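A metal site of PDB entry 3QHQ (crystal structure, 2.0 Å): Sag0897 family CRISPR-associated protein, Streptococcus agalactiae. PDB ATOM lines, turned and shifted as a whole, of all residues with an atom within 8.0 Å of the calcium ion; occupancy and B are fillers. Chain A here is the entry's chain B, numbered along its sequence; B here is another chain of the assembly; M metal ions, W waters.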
ATOM      1  N   VAL A  71       7.374 -14.934  11.385  1.00  0.00           N
ATOM      2  CA  VAL A  71       6.336 -14.129  12.074  1.00  0.00           C
ATOM      3  C   VAL A  71       5.155 -14.960  12.577  1.00  0.00           C
ATOM      4  O   VAL A  71       4.182 -14.411  13.094  1.00  0.00           O
ATOM      5  CB  VAL A  71       5.807 -12.964  11.192  1.00  0.00           C
ATOM      6  CG1 VAL A  71       6.875 -11.889  10.994  1.00  0.00           C
ATOM      7  CG2 VAL A  71       5.251 -13.483   9.869  1.00  0.00           C
ATOM      8  N   ILE A 138      -0.576 -15.294   9.905  1.00  0.00           N
ATOM      9  CA  ILE A 138      -0.112 -14.309   8.932  1.00  0.00           C
ATOM     10  C   ILE A 138       0.195 -14.995   7.600  1.00  0.00           C
ATOM     11  O   ILE A 138       0.888 -16.026   7.564  1.00  0.00           O
ATOM     12  CB  ILE A 138       1.119 -13.534   9.476  1.00  0.00           C
ATOM     13  CG1 ILE A 138       0.744 -12.776  10.753  1.00  0.00           C
ATOM     14  CG2 ILE A 138       1.652 -12.547   8.425  1.00  0.00           C
ATOM     15  CD1 ILE A 138       1.910 -12.193  11.509  1.00  0.00           C
ATOM     16  N   GLU A 139      -0.356 -14.444   6.520  1.00  0.00           N
ATOM     17  CA  GLU A 139      -0.013 -14.911   5.177  1.00  0.00           C
ATOM     18  C   GLU A 139       1.368 -14.370   4.860  1.00  0.00           C
ATOM     19  O   GLU A 139       1.603 -13.168   4.981  1.00  0.00           O
ATOM     20  CB  GLU A 139      -1.038 -14.390   4.161  1.00  0.00           C
ATOM     21  CG  GLU A 139      -0.963 -15.050   2.776  1.00  0.00           C
ATOM     22  CD  GLU A 139       0.152 -14.482   1.887  1.00  0.00           C
ATOM     23  OE1 GLU A 139       0.755 -13.457   2.242  1.00  0.00           O
ATOM     24  OE2 GLU A 139       0.406 -15.071   0.822  1.00  0.00           O
ATOM     25  N   THR A 140       2.284 -15.261   4.454  1.00  0.00           N
ATOM     26  CA  THR A 140       3.649 -14.842   4.095  1.00  0.00           C
ATOM     27  C   THR A 140       4.101 -15.313   2.708  1.00  0.00           C
ATOM     28  O   THR A 140       5.054 -14.785   2.164  1.00  0.00           O
ATOM     29  CB  THR A 140       4.712 -15.280   5.142  1.00  0.00           C
ATOM     30  OG1 THR A 140       4.724 -16.707   5.264  1.00  0.00           O
ATOM     31  CG2 THR A 140       4.447 -14.642   6.504  1.00  0.00           C
ATOM     32  N   GLN A 141       3.406 -16.310   2.157  1.00  0.00           N
ATOM     33  CA  GLN A 141       3.844 -16.970   0.920  1.00  0.00           C
ATOM     34  C   GLN A 141       4.068 -15.979  -0.229  1.00  0.00           C
ATOM     35  O   GLN A 141       5.116 -16.005  -0.886  1.00  0.00           O
ATOM     36  CB  GLN A 141       2.831 -18.039   0.512  1.00  0.00           C
ATOM     37  CG  GLN A 141       3.355 -19.056  -0.489  1.00  0.00           C
ATOM     38  CD  GLN A 141       2.390 -20.217  -0.694  1.00  0.00           C
ATOM     39  OE1 GLN A 141       1.292 -20.061  -1.231  1.00  0.00           O
ATOM     40  NE2 GLN A 141       2.807 -21.410  -0.255  1.00  0.00           N
ATOM     41  N   SER A 142       3.091 -15.100  -0.443  1.00  0.00           N
ATOM     42  CA  SER A 142       3.134 -14.148  -1.552  1.00  0.00           C
ATOM     43  C   SER A 142       3.887 -12.843  -1.252  1.00  0.00           C
ATOM     44  O   SER A 142       4.009 -11.985  -2.137  1.00  0.00           O
ATOM     45  CB  SER A 142       1.717 -13.823  -2.019  1.00  0.00           C
ATOM     46  OG  SER A 142       0.990 -13.197  -0.968  1.00  0.00           O
ATOM     47  N   ASP A 143       4.392 -12.704  -0.022  1.00  0.00           N
ATOM     48  CA  ASP A 143       5.015 -11.457   0.451  1.00  0.00           C
ATOM     49  C   ASP A 143       6.031 -10.860  -0.505  1.00  0.00           C
ATOM     50  O   ASP A 143       6.947 -11.548  -0.966  1.00  0.00           O
ATOM     51  CB  ASP A 143       5.744 -11.681   1.780  1.00  0.00           C
ATOM     52  CG  ASP A 143       4.802 -11.759   2.958  1.00  0.00           C
ATOM     53  OD1 ASP A 143       3.573 -11.693   2.760  1.00  0.00           O
ATOM     54  OD2 ASP A 143       5.307 -11.900   4.099  1.00  0.00           O
ATOM     55  N   THR A 144       5.886  -9.563  -0.770  1.00  0.00           N
ATOM     56  CA  THR A 144       7.008  -8.772  -1.256  1.00  0.00           C
ATOM     57  C   THR A 144       7.865  -8.469  -0.017  1.00  0.00           C
ATOM     58  O   THR A 144       7.406  -8.671   1.102  1.00  0.00           O
ATOM     59  CB  THR A 144       6.551  -7.447  -1.892  1.00  0.00           C
ATOM     60  OG1 THR A 144       5.866  -6.663  -0.909  1.00  0.00           O
ATOM     61  CG2 THR A 144       5.632  -7.714  -3.084  1.00  0.00           C
ATOM     62  N   GLU A 147       6.086  -5.887   2.060  1.00  0.00           N
ATOM     63  CA  GLU A 147       4.959  -6.493   2.788  1.00  0.00           C
ATOM     64  C   GLU A 147       5.427  -7.222   4.047  1.00  0.00           C
ATOM     65  O   GLU A 147       4.801  -7.091   5.105  1.00  0.00           O
ATOM     66  CB  GLU A 147       4.147  -7.411   1.877  1.00  0.00           C
ATOM     67  CG  GLU A 147       3.173  -6.654   0.937  1.00  0.00           C
ATOM     68  CD  GLU A 147       2.471  -7.571  -0.060  1.00  0.00           C
ATOM     69  OE1 GLU A 147       2.954  -8.693  -0.304  1.00  0.00           O
ATOM     70  OE2 GLU A 147       1.426  -7.164  -0.598  1.00  0.00           O
ATOM     71  N   LYS A 148       6.512  -7.977   3.926  1.00  0.00           N
ATOM     72  CA  LYS A 148       7.075  -8.719   5.063  1.00  0.00           C
ATOM     73  C   LYS A 148       7.687  -7.804   6.117  1.00  0.00           C
ATOM     74  O   LYS A 148       7.538  -8.053   7.313  1.00  0.00           O
ATOM     75  CB  LYS A 148       8.084  -9.789   4.586  1.00  0.00           C
ATOM     76  CG  LYS A 148       8.713 -10.611   5.720  1.00  0.00           C
ATOM     77  CD  LYS A 148       7.668 -11.331   6.598  1.00  0.00           C
ATOM     78  CE  LYS A 148       8.316 -12.370   7.501  1.00  0.00           C
ATOM     79  NZ  LYS A 148       9.022 -13.473   6.723  1.00  0.00           N
ATOM     80  N   GLU A 151       4.751  -6.629   8.076  1.00  0.00           N
ATOM     81  CA  GLU A 151       4.306  -7.711   8.966  1.00  0.00           C
ATOM     82  C   GLU A 151       5.222  -7.855  10.197  1.00  0.00           C
ATOM     83  O   GLU A 151       4.738  -8.081  11.312  1.00  0.00           O
ATOM     84  CB  GLU A 151       4.218  -9.045   8.188  1.00  0.00           C
ATOM     85  CG  GLU A 151       3.013  -9.148   7.245  1.00  0.00           C
ATOM     86  CD  GLU A 151       3.193 -10.182   6.144  1.00  0.00           C
ATOM     87  OE1 GLU A 151       4.259 -10.850   6.125  1.00  0.00           O
ATOM     88  OE2 GLU A 151       2.288 -10.329   5.279  1.00  0.00           O
ATOM     89  N   LEU B 118      -3.211  -6.847  10.270  1.00  0.00           N
ATOM     90  CA  LEU B 118      -2.316  -7.862   9.708  1.00  0.00           C
ATOM     91  C   LEU B 118      -2.954  -8.537   8.510  1.00  0.00           C
ATOM     92  O   LEU B 118      -4.169  -8.670   8.439  1.00  0.00           O
ATOM     93  CB  LEU B 118      -1.957  -8.928  10.751  1.00  0.00           C
ATOM     94  CG  LEU B 118      -0.828  -8.608  11.720  1.00  0.00           C
ATOM     95  CD1 LEU B 118      -0.947  -9.500  12.951  1.00  0.00           C
ATOM     96  CD2 LEU B 118       0.528  -8.770  11.046  1.00  0.00           C
ATOM     97  N   ASP B 119      -2.109  -8.959   7.561  1.00  0.00           N
ATOM     98  CA  ASP B 119      -2.565  -9.753   6.434  1.00  0.00           C
ATOM     99  C   ASP B 119      -2.711 -11.198   6.882  1.00  0.00           C
ATOM    100  O   ASP B 119      -1.728 -11.938   7.013  1.00  0.00           O
ATOM    101  CB  ASP B 119      -1.602  -9.623   5.262  1.00  0.00           C
ATOM    102  CG  ASP B 119      -1.999 -10.474   4.078  1.00  0.00           C
ATOM    103  OD1 ASP B 119      -3.224 -10.622   3.827  1.00  0.00           O
ATOM    104  OD2 ASP B 119      -1.109 -11.011   3.414  1.00  0.00           O
ATOM    105  N   LEU B 120      -3.952 -11.595   7.137  1.00  0.00           N
ATOM    106  CA  LEU B 120      -4.231 -12.873   7.776  1.00  0.00           C
ATOM    107  C   LEU B 120      -4.860 -13.884   6.825  1.00  0.00           C
ATOM    108  O   LEU B 120      -5.650 -13.529   5.945  1.00  0.00           O
ATOM    109  CB  LEU B 120      -5.123 -12.670   9.007  1.00  0.00           C
ATOM    110  CG  LEU B 120      -4.545 -11.830  10.152  1.00  0.00           C
ATOM    111  CD1 LEU B 120      -5.605 -11.579  11.212  1.00  0.00           C
ATOM    112  CD2 LEU B 120      -3.297 -12.500  10.766  1.00  0.00           C
ATOM    113  N   GLU B 121      -4.481 -15.128   7.015  1.00  0.00           N
ATOM    114  CA  GLU B 121      -5.076 -16.261   6.321  1.00  0.00           C
ATOM    115  C   GLU B 121      -5.461 -17.320   7.348  1.00  0.00           C
ATOM    116  O   GLU B 121      -5.149 -17.172   8.545  1.00  0.00           O
ATOM    117  CB  GLU B 121      -4.112 -16.828   5.268  1.00  0.00           C
ATOM    118  CG  GLU B 121      -2.853 -17.488   5.847  1.00  0.00           C
ATOM    119  CD  GLU B 121      -1.988 -18.135   4.786  1.00  0.00           C
ATOM    120  OE1 GLU B 121      -2.472 -18.333   3.650  1.00  0.00           O
ATOM    121  OE2 GLU B 121      -0.819 -18.453   5.078  1.00  0.00           O
HETATM  122 CA    CA M   1       1.356 -11.331   3.341  1.00  0.00          CA
HETATM  123  O   HOH W   1       1.237 -10.771   0.915  1.00  0.00           O
HETATM  124  O   HOH W   2       1.076  -8.839   3.185  1.00  0.00           O
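The side-chain carboxylate of Glu 139 is in hydrogen-bond range of the side-chain hydroxyl of Ser 142 (2.7 Å).
Of the 15 residues printed, 4 come within 4 Å of the calcium ion.
The calcium ion is bound by the side-chain carboxylate of Asp 143 (2.3 Å), the side-chain carboxylate of Glu 151 (2.4 Å), the side-chain carboxylate of Glu 139 (2.5 Å), the backbone carbonyl oxygen of Glu 139 (2.5 Å), the side-chain carboxylate of Asp 119 of chain B (2.5 Å), water W1 (2.5 Å) and water W2 (2.5 Å).
Water W1 lies within hydrogen-bond range of OE1 of Glu 147 (3.0 Å) and OG of Ser 142 (3.1 Å).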
